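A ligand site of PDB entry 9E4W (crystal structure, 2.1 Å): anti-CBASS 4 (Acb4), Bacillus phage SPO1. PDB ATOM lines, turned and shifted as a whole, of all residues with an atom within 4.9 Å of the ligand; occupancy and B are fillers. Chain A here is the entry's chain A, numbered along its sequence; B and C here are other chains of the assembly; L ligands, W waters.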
ATOM      1  N   LYS A  37     -30.801   7.907   5.988  1.00  0.00           N
ATOM      2  CA  LYS A  37     -30.007   7.375   7.093  1.00  0.00           C
ATOM      3  C   LYS A  37     -30.368   5.954   7.500  1.00  0.00           C
ATOM      4  O   LYS A  37     -29.548   5.299   8.158  1.00  0.00           O
ATOM      5  CB  LYS A  37     -30.149   8.280   8.327  1.00  0.00           C
ATOM      6  CG  LYS A  37     -29.636   9.691   8.133  1.00  0.00           C
ATOM      7  CD  LYS A  37     -30.300  10.667   9.093  1.00  0.00           C
ATOM      8  CE  LYS A  37     -29.904  10.405  10.544  1.00  0.00           C
ATOM      9  NZ  LYS A  37     -28.458  10.659  10.788  1.00  0.00           N
ATOM     10  N   THR A  39     -31.811   1.879   7.122  1.00  0.00           N
ATOM     11  CA  THR A  39     -31.973   0.652   6.369  1.00  0.00           C
ATOM     12  C   THR A  39     -32.980  -0.240   7.092  1.00  0.00           C
ATOM     13  O   THR A  39     -32.947  -0.340   8.324  1.00  0.00           O
ATOM     14  CB  THR A  39     -30.643  -0.086   6.213  1.00  0.00           C
ATOM     15  OG1 THR A  39     -29.664   0.811   5.662  1.00  0.00           O
ATOM     16  CG2 THR A  39     -30.797  -1.283   5.279  1.00  0.00           C
ATOM     17  N   THR A  54     -34.224  -2.584  11.942  1.00  0.00           N
ATOM     18  CA  THR A  54     -33.817  -1.336  11.312  1.00  0.00           C
ATOM     19  C   THR A  54     -32.479  -0.884  11.861  1.00  0.00           C
ATOM     20  O   THR A  54     -32.043  -1.304  12.933  1.00  0.00           O
ATOM     21  CB  THR A  54     -34.851  -0.223  11.513  1.00  0.00           C
ATOM     22  OG1 THR A  54     -34.931   0.117  12.911  1.00  0.00           O
ATOM     23  CG2 THR A  54     -36.230  -0.649  11.026  1.00  0.00           C
ATOM     24  N   SER A  55     -31.831   0.001  11.108  1.00  0.00           N
ATOM     25  CA  SER A  55     -30.611   0.682  11.528  1.00  0.00           C
ATOM     26  C   SER A  55     -30.689   2.126  11.055  1.00  0.00           C
ATOM     27  O   SER A  55     -31.366   2.422  10.068  1.00  0.00           O
ATOM     28  CB  SER A  55     -29.359   0.021  10.958  1.00  0.00           C
ATOM     29  OG  SER A  55     -29.314   0.147   9.549  1.00  0.00           O
ATOM     30  N   SER A  56     -29.999   3.023  11.765  1.00  0.00           N
ATOM     31  CA  SER A  56     -30.022   4.440  11.417  1.00  0.00           C
ATOM     32  C   SER A  56     -28.659   5.037  11.726  1.00  0.00           C
ATOM     33  O   SER A  56     -28.291   5.186  12.893  1.00  0.00           O
ATOM     34  CB  SER A  56     -31.122   5.170  12.171  1.00  0.00           C
ATOM     35  OG  SER A  56     -32.402   4.677  11.812  1.00  0.00           O
ATOM     36  N   VAL A  57     -27.910   5.390  10.673  1.00  0.00           N
ATOM     37  CA  VAL A  57     -26.595   5.971  10.864  1.00  0.00           C
ATOM     38  C   VAL A  57     -26.742   7.405  11.377  1.00  0.00           C
ATOM     39  O   VAL A  57     -27.667   8.130  10.998  1.00  0.00           O
ATOM     40  CB  VAL A  57     -25.779   5.911   9.552  1.00  0.00           C
ATOM     41  CG1 VAL A  57     -26.440   6.760   8.466  1.00  0.00           C
ATOM     42  CG2 VAL A  57     -24.336   6.321   9.781  1.00  0.00           C
ATOM     43  N   TYR A  58     -25.824   7.807  12.261  1.00  0.00           N
ATOM     44  CA  TYR A  58     -25.904   9.130  12.864  1.00  0.00           C
ATOM     45  C   TYR A  58     -25.471  10.219  11.882  1.00  0.00           C
ATOM     46  O   TYR A  58     -26.137  11.258  11.758  1.00  0.00           O
ATOM     47  CB  TYR A  58     -25.055   9.180  14.129  1.00  0.00           C
ATOM     48  CG  TYR A  58     -25.108  10.503  14.869  1.00  0.00           C
ATOM     49  CD1 TYR A  58     -26.315  11.097  15.187  1.00  0.00           C
ATOM     50  CD2 TYR A  58     -23.940  11.126  15.270  1.00  0.00           C
ATOM     51  CE1 TYR A  58     -26.370  12.300  15.866  1.00  0.00           C
ATOM     52  CE2 TYR A  58     -23.971  12.329  15.954  1.00  0.00           C
ATOM     53  CZ  TYR A  58     -25.186  12.917  16.252  1.00  0.00           C
ATOM     54  OH  TYR A  58     -25.222  14.106  16.929  1.00  0.00           O
ATOM     55  N   LYS A  59     -24.371   9.997  11.178  1.00  0.00           N
ATOM     56  CA  LYS A  59     -23.855  10.934  10.194  1.00  0.00           C
ATOM     57  C   LYS A  59     -24.219  10.411   8.808  1.00  0.00           C
ATOM     58  O   LYS A  59     -23.683   9.391   8.351  1.00  0.00           O
ATOM     59  CB  LYS A  59     -22.340  11.107  10.341  1.00  0.00           C
ATOM     60  CG  LYS A  59     -21.937  11.802  11.632  1.00  0.00           C
ATOM     61  CD  LYS A  59     -20.461  11.590  11.947  1.00  0.00           C
ATOM     62  CE  LYS A  59     -20.014  12.486  13.086  1.00  0.00           C
ATOM     63  NZ  LYS A  59     -20.899  12.381  14.278  1.00  0.00           N
ATOM     64  N   ASN A  62     -21.714   9.347   6.187  1.00  0.00           N
ATOM     65  CA  ASN A  62     -20.988   8.104   6.398  1.00  0.00           C
ATOM     66  C   ASN A  62     -21.822   6.880   6.029  1.00  0.00           C
ATOM     67  O   ASN A  62     -21.461   5.754   6.401  1.00  0.00           O
ATOM     68  CB  ASN A  62     -20.518   7.994   7.845  1.00  0.00           C
ATOM     69  CG  ASN A  62     -19.508   9.070   8.211  1.00  0.00           C
ATOM     70  OD1 ASN A  62     -18.919   9.704   7.345  1.00  0.00           O
ATOM     71  ND2 ASN A  62     -19.308   9.267   9.511  1.00  0.00           N
ATOM     72  N   PHE A  63     -22.929   7.062   5.307  1.00  0.00           N
ATOM     73  CA  PHE A  63     -23.810   5.956   4.989  1.00  0.00           C
ATOM     74  C   PHE A  63     -23.095   4.911   4.146  1.00  0.00           C
ATOM     75  O   PHE A  63     -22.360   5.242   3.214  1.00  0.00           O
ATOM     76  CB  PHE A  63     -25.055   6.458   4.259  1.00  0.00           C
ATOM     77  CG  PHE A  63     -26.153   5.432   4.158  1.00  0.00           C
ATOM     78  CD1 PHE A  63     -26.166   4.484   3.142  1.00  0.00           C
ATOM     79  CD2 PHE A  63     -27.169   5.408   5.101  1.00  0.00           C
ATOM     80  CE1 PHE A  63     -27.172   3.547   3.064  1.00  0.00           C
ATOM     81  CE2 PHE A  63     -28.187   4.464   5.020  1.00  0.00           C
ATOM     82  CZ  PHE A  63     -28.178   3.538   3.998  1.00  0.00           C
ATOM     83  N   ASN A  64     -23.314   3.646   4.475  1.00  0.00           N
ATOM     84  CA  ASN A  64     -22.708   2.532   3.772  1.00  0.00           C
ATOM     85  C   ASN A  64     -23.711   1.383   3.750  1.00  0.00           C
ATOM     86  O   ASN A  64     -24.153   0.938   4.814  1.00  0.00           O
ATOM     87  CB  ASN A  64     -21.404   2.097   4.434  1.00  0.00           C
ATOM     88  CG  ASN A  64     -20.809   0.869   3.797  1.00  0.00           C
ATOM     89  OD1 ASN A  64     -21.159  -0.261   4.158  1.00  0.00           O
ATOM     90  ND2 ASN A  64     -19.901   1.072   2.849  1.00  0.00           N
ATOM     91  N   ILE A  67     -22.880  -1.959   6.011  1.00  0.00           N
ATOM     92  CA  ILE A  67     -23.008  -1.827   7.460  1.00  0.00           C
ATOM     93  C   ILE A  67     -24.474  -1.641   7.846  1.00  0.00           C
ATOM     94  O   ILE A  67     -24.934  -2.186   8.862  1.00  0.00           O
ATOM     95  CB  ILE A  67     -22.136  -0.666   7.985  1.00  0.00           C
ATOM     96  CG1 ILE A  67     -20.693  -0.845   7.498  1.00  0.00           C
ATOM     97  CG2 ILE A  67     -22.184  -0.602   9.498  1.00  0.00           C
ATOM     98  CD1 ILE A  67     -19.749   0.227   8.002  1.00  0.00           C
ATOM     99  N   GLY A  68     -25.232  -0.904   7.038  1.00  0.00           N
ATOM    100  CA  GLY A  68     -26.645  -0.722   7.324  1.00  0.00           C
ATOM    101  C   GLY A  68     -27.423  -2.017   7.269  1.00  0.00           C
ATOM    102  O   GLY A  68     -28.296  -2.267   8.093  1.00  0.00           O
ATOM    103  N   THR A  71     -26.345  -4.214  10.330  1.00  0.00           N
ATOM    104  CA  THR A  71     -26.923  -3.747  11.592  1.00  0.00           C
ATOM    105  C   THR A  71     -28.426  -3.991  11.624  1.00  0.00           C
ATOM    106  O   THR A  71     -28.966  -4.363  12.678  1.00  0.00           O
ATOM    107  CB  THR A  71     -26.614  -2.262  11.791  1.00  0.00           C
ATOM    108  OG1 THR A  71     -25.200  -2.049  11.678  1.00  0.00           O
ATOM    109  CG2 THR A  71     -27.069  -1.797  13.158  1.00  0.00           C
ATOM    110  N   PHE B  49     -33.735  14.358  11.706  1.00  0.00           N
ATOM    111  CA  PHE B  49     -33.699  13.157  12.517  1.00  0.00           C
ATOM    112  C   PHE B  49     -34.862  12.251  12.148  1.00  0.00           C
ATOM    113  O   PHE B  49     -36.005  12.710  11.998  1.00  0.00           O
ATOM    114  CB  PHE B  49     -33.759  13.525  14.003  1.00  0.00           C
ATOM    115  CG  PHE B  49     -33.642  12.342  14.928  1.00  0.00           C
ATOM    116  CD1 PHE B  49     -32.392  11.871  15.304  1.00  0.00           C
ATOM    117  CD2 PHE B  49     -34.766  11.721  15.439  1.00  0.00           C
ATOM    118  CE1 PHE B  49     -32.275  10.794  16.160  1.00  0.00           C
ATOM    119  CE2 PHE B  49     -34.662  10.650  16.292  1.00  0.00           C
ATOM    120  CZ  PHE B  49     -33.418  10.180  16.660  1.00  0.00           C
ATOM    121  N   GLU B  50     -34.589  10.955  11.987  1.00  0.00           N
ATOM    122  CA  GLU B  50     -35.554  10.010  11.444  1.00  0.00           C
ATOM    123  C   GLU B  50     -36.169   9.174  12.567  1.00  0.00           C
ATOM    124  O   GLU B  50     -35.450   8.683  13.442  1.00  0.00           O
ATOM    125  CB  GLU B  50     -34.902   9.105  10.411  1.00  0.00           C
ATOM    126  CG  GLU B  50     -34.269   9.850   9.249  1.00  0.00           C
ATOM    127  CD  GLU B  50     -33.575   8.926   8.274  1.00  0.00           C
ATOM    128  OE1 GLU B  50     -33.799   7.705   8.366  1.00  0.00           O
ATOM    129  OE2 GLU B  50     -32.809   9.420   7.416  1.00  0.00           O
ATOM    130  N   VAL B  51     -37.494   9.030  12.518  1.00  0.00           N
ATOM    131  CA  VAL B  51     -38.235   8.182  13.445  1.00  0.00           C
ATOM    132  C   VAL B  51     -39.039   7.190  12.613  1.00  0.00           C
ATOM    133  O   VAL B  51     -39.845   7.592  11.764  1.00  0.00           O
ATOM    134  CB  VAL B  51     -39.159   9.005  14.360  1.00  0.00           C
ATOM    135  CG1 VAL B  51     -39.790   8.112  15.419  1.00  0.00           C
ATOM    136  CG2 VAL B  51     -38.387  10.139  15.016  1.00  0.00           C
ATOM    137  N   PHE B  83     -39.173  11.084  22.082  1.00  0.00           N
ATOM    138  CA  PHE B  83     -38.105  12.047  21.837  1.00  0.00           C
ATOM    139  C   PHE B  83     -38.518  13.448  22.253  1.00  0.00           C
ATOM    140  O   PHE B  83     -37.687  14.232  22.720  1.00  0.00           O
ATOM    141  CB  PHE B  83     -37.699  12.027  20.366  1.00  0.00           C
ATOM    142  CG  PHE B  83     -36.975  10.774  19.937  1.00  0.00           C
ATOM    143  CD1 PHE B  83     -35.669  10.540  20.336  1.00  0.00           C
ATOM    144  CD2 PHE B  83     -37.605   9.839  19.122  1.00  0.00           C
ATOM    145  CE1 PHE B  83     -35.010   9.390  19.934  1.00  0.00           C
ATOM    146  CE2 PHE B  83     -36.946   8.689  18.721  1.00  0.00           C
ATOM    147  CZ  PHE B  83     -35.634   8.469  19.127  1.00  0.00           C
ATOM    148  N   ILE C  81     -28.689   6.143  23.576  1.00  0.00           N
ATOM    149  CA  ILE C  81     -27.882   6.718  22.505  1.00  0.00           C
ATOM    150  C   ILE C  81     -28.774   7.344  21.444  1.00  0.00           C
ATOM    151  O   ILE C  81     -28.438   8.390  20.870  1.00  0.00           O
ATOM    152  CB  ILE C  81     -26.946   5.639  21.908  1.00  0.00           C
ATOM    153  CG1 ILE C  81     -25.846   5.285  22.909  1.00  0.00           C
ATOM    154  CG2 ILE C  81     -26.347   6.108  20.597  1.00  0.00           C
ATOM    155  CD1 ILE C  81     -24.991   4.109  22.482  1.00  0.00           C
ATOM    156  N   LYS C  82     -29.934   6.728  21.170  1.00  0.00           N
ATOM    157  CA  LYS C  82     -30.880   7.322  20.238  1.00  0.00           C
ATOM    158  C   LYS C  82     -31.311   8.708  20.697  1.00  0.00           C
ATOM    159  O   LYS C  82     -31.373   9.653  19.905  1.00  0.00           O
ATOM    160  CB  LYS C  82     -32.111   6.412  20.091  1.00  0.00           C
ATOM    161  CG  LYS C  82     -31.797   4.992  19.670  1.00  0.00           C
ATOM    162  CD  LYS C  82     -33.076   4.185  19.549  1.00  0.00           C
ATOM    163  CE  LYS C  82     -32.782   2.706  19.335  1.00  0.00           C
ATOM    164  NZ  LYS C  82     -31.979   2.476  18.107  1.00  0.00           N
ATOM    165  N   ALA C  85     -28.628  11.071  20.015  1.00  0.00           N
ATOM    166  CA  ALA C  85     -28.575  11.423  18.605  1.00  0.00           C
ATOM    167  C   ALA C  85     -29.674  12.410  18.238  1.00  0.00           C
ATOM    168  O   ALA C  85     -29.487  13.239  17.335  1.00  0.00           O
ATOM    169  CB  ALA C  85     -28.673  10.165  17.742  1.00  0.00           C
ATOM    170  N   LEU C  90     -24.979  13.391  21.246  1.00  0.00           N
ATOM    171  CA  LEU C  90     -24.130  12.300  20.795  1.00  0.00           C
ATOM    172  C   LEU C  90     -22.848  12.830  20.159  1.00  0.00           C
ATOM    173  O   LEU C  90     -21.791  12.204  20.298  1.00  0.00           O
ATOM    174  CB  LEU C  90     -24.893  11.410  19.802  1.00  0.00           C
ATOM    175  CG  LEU C  90     -24.145  10.180  19.283  1.00  0.00           C
ATOM    176  CD1 LEU C  90     -23.690   9.314  20.446  1.00  0.00           C
ATOM    177  CD2 LEU C  90     -25.017   9.377  18.332  1.00  0.00           C
ATOM    178  N   LEU C  94     -18.944  11.774  21.086  1.00  0.00           N
ATOM    179  CA  LEU C  94     -18.008  11.264  20.097  1.00  0.00           C
ATOM    180  C   LEU C  94     -16.717  12.072  20.060  1.00  0.00           C
ATOM    181  O   LEU C  94     -15.663  11.542  19.703  1.00  0.00           O
ATOM    182  CB  LEU C  94     -18.655  11.224  18.719  1.00  0.00           C
ATOM    183  CG  LEU C  94     -19.860  10.293  18.589  1.00  0.00           C
ATOM    184  CD1 LEU C  94     -20.409  10.314  17.176  1.00  0.00           C
ATOM    185  CD2 LEU C  94     -19.493   8.877  19.004  1.00  0.00           C
HETATM  186  O1  LIG L   1     -31.813   9.530  12.871  1.00  0.00           O
HETATM  187  C1  LIG L   1     -31.884   8.657  13.699  1.00  0.00           C
HETATM  188  N1  LIG L   1     -33.145   8.152  14.073  1.00  0.00           N
HETATM  189  C2  LIG L   1     -33.235   7.114  15.071  1.00  0.00           C
HETATM  190  N2  LIG L   1     -34.529   6.600  15.462  1.00  0.00           N
HETATM  191  N3  LIG L   1     -32.032   6.590  15.678  1.00  0.00           N
HETATM  192  C3  LIG L   1     -30.732   7.104  15.295  1.00  0.00           C
HETATM  193  C4  LIG L   1     -30.636   8.107  14.334  1.00  0.00           C
HETATM  194  N4  LIG L   1     -29.304   8.380  14.185  1.00  0.00           N
HETATM  195  C5  LIG L   1     -28.618   7.591  15.006  1.00  0.00           C
HETATM  196  N5  LIG L   1     -29.453   6.805  15.693  1.00  0.00           N
HETATM  197  C6  LIG L   1     -29.095   5.815  16.665  1.00  0.00           C
HETATM  198  C7  LIG L   1     -29.162   4.655  16.161  1.00  0.00           C
HETATM  199  O2  LIG L   1     -29.960   3.757  17.033  1.00  0.00           O
HETATM  200  O3  LIG L   1     -27.523   6.052  17.188  1.00  0.00           O
HETATM  201  C8  LIG L   1     -26.962   4.874  17.196  1.00  0.00           C
HETATM  202  C9  LIG L   1     -25.461   5.007  16.900  1.00  0.00           C
HETATM  203  O4  LIG L   1     -25.321   5.681  15.617  1.00  0.00           O
HETATM  204  P1  LIG L   1     -23.877   5.645  14.949  1.00  0.00           P
HETATM  205  O5  LIG L   1     -23.267   4.138  14.791  1.00  0.00           O
HETATM  206  O6  LIG L   1     -24.098   6.141  13.538  1.00  0.00           O
HETATM  207  O7  LIG L   1     -22.911   6.618  15.558  1.00  0.00           O
HETATM  208  C10 LIG L   1     -27.668   4.100  16.082  1.00  0.00           C
HETATM  209  O8  LIG L   1     -27.650   2.804  16.336  1.00  0.00           O
HETATM  210  P2  LIG L   1     -27.699   1.791  15.180  1.00  0.00           P
HETATM  211  O9  LIG L   1     -27.942   0.487  15.853  1.00  0.00           O
HETATM  212  O10 LIG L   1     -28.862   1.951  14.255  1.00  0.00           O
HETATM  213  O11 LIG L   1     -26.302   1.583  14.427  1.00  0.00           O
HETATM  214  C11 LIG L   1     -25.092   1.504  15.228  1.00  0.00           C
HETATM  215  C12 LIG L   1     -23.896   1.692  14.305  1.00  0.00           C
HETATM  216  O12 LIG L   1     -24.014   0.966  13.269  1.00  0.00           O
HETATM  217  C13 LIG L   1     -23.831   3.214  13.743  1.00  0.00           C
HETATM  218  C14 LIG L   1     -23.070   3.149  12.774  1.00  0.00           C
HETATM  219  O13 LIG L   1     -21.636   3.196  13.238  1.00  0.00           O
HETATM  220  C15 LIG L   1     -23.380   1.760  12.144  1.00  0.00           C
HETATM  221  N6  LIG L   1     -24.220   1.892  11.134  1.00  0.00           N
HETATM  222  C16 LIG L   1     -25.515   1.579  11.130  1.00  0.00           C
HETATM  223  N7  LIG L   1     -26.050   1.840   9.938  1.00  0.00           N
HETATM  224  C17 LIG L   1     -25.071   2.358   9.131  1.00  0.00           C
HETATM  225  C18 LIG L   1     -23.892   2.391   9.903  1.00  0.00           C
HETATM  226  N8  LIG L   1     -22.756   2.856   9.332  1.00  0.00           N
HETATM  227  C19 LIG L   1     -22.748   3.284   8.080  1.00  0.00           C
HETATM  228  N9  LIG L   1     -23.848   3.254   7.332  1.00  0.00           N
HETATM  229  C20 LIG L   1     -25.027   2.815   7.792  1.00  0.00           C
HETATM  230  N10 LIG L   1     -26.191   2.812   6.953  1.00  0.00           N
HETATM  231  O   HOH W   1     -28.702   3.030  19.552  1.00  0.00           O
HETATM  232  O   HOH W   2     -28.763   2.249   8.161  1.00  0.00           O
HETATM  233  O   HOH W   3     -23.117  -1.926  13.449  1.00  0.00           O
HETATM  234  O   HOH W   4     -31.385   1.575  15.253  1.00  0.00           O
HETATM  235  O   HOH W   5     -29.070   0.396  18.358  1.00  0.00           O
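The backbone NH (N) of Glu 50 of chain B is in hydrogen-bond range of an oxygen (O1) of the ligand, at 3.2 Å.
The side-chain amino group (NZ) of Lys 82 of chain C is in hydrogen-bond range of an oxygen (O2) of the ligand (2.6 Å).
N of Tyr 58 sits at hydrogen-bond distance from O6 of the ligand (2.7 Å).
N of Ser 56 sits at hydrogen-bond distance from O10 of the ligand, at 2.9 Å.
The backbone carbonyl oxygen (O) of Asn 64 is in hydrogen-bond range of a nitrogen (N10) of the ligand, 3.5 Å away.
A nitrogen (N9) of the ligand is in hydrogen-bond range of the backbone NH of Asn 64, at 2.9 Å.
The backbone carbonyl oxygen of Glu 50 of chain B lies within hydrogen-bond range of a nitrogen (N1) of the ligand, at 2.4 Å.
The backbone carbonyl oxygen of Gly 68 sits at hydrogen-bond distance from the side-chain hydroxyl of Ser 55, 3.0 Å away.
The backbone NH of Lys 37 is in hydrogen-bond range of the side-chain carboxylate of Glu 50 of chain B, 2.9 Å away.
NZ of Lys 37 is in hydrogen-bond range of O of Val 57 (2.7 Å).
N of Ile 67 sits at hydrogen-bond distance from OD1 of Asn 64, 3.0 Å away.
The backbone carbonyl oxygen (O) of Tyr 58 sits at hydrogen-bond distance from the side-chain amino group (NZ) of Lys 37 (2.6 Å).
N of Ser 55 is in hydrogen-bond range of O of Thr 39 (3.0 Å).
The backbone carbonyl oxygen (O) of Ile 67 lies within hydrogen-bond range of the side-chain hydroxyl (OG1) of Thr 71, 2.8 Å away.
Residues that only touch the ligand: Lys 37, Ser 55, Val 57, Asn 62, Phe 63, Ile 67, Gly 68, Thr 71, Phe 49 of chain B, Ile 81 of chain C and Ala 85 of chain C.
Hydrophobic or aromatic side chains within 4 Å of the ligand: Val 57, Tyr 58, Phe 63, Ile 67, Phe 49 of chain B, Ile 81 of chain C and Ala 85 of chain C.
Of the 23 residues printed, 16 come within 4 Å of the ligand.
Along chain A the residues within 4 Å of the ligand span positions 37 to 71.
Water W4 lies within hydrogen-bond range of O10 of the ligand (2.7 Å) and NZ of Lys 82 of chain C (3.1 Å).
Water W2 lies within hydrogen-bond range of OG of Ser 55 (2.6 Å), N10 of the ligand (2.9 Å), OG1 of Thr 39 (3.0 Å) and O of Lys 37 (3.1 Å).
Water W3 lies within hydrogen-bond range of OG1 of Thr 71 (2.7 Å) and O12 of the ligand (3.0 Å).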
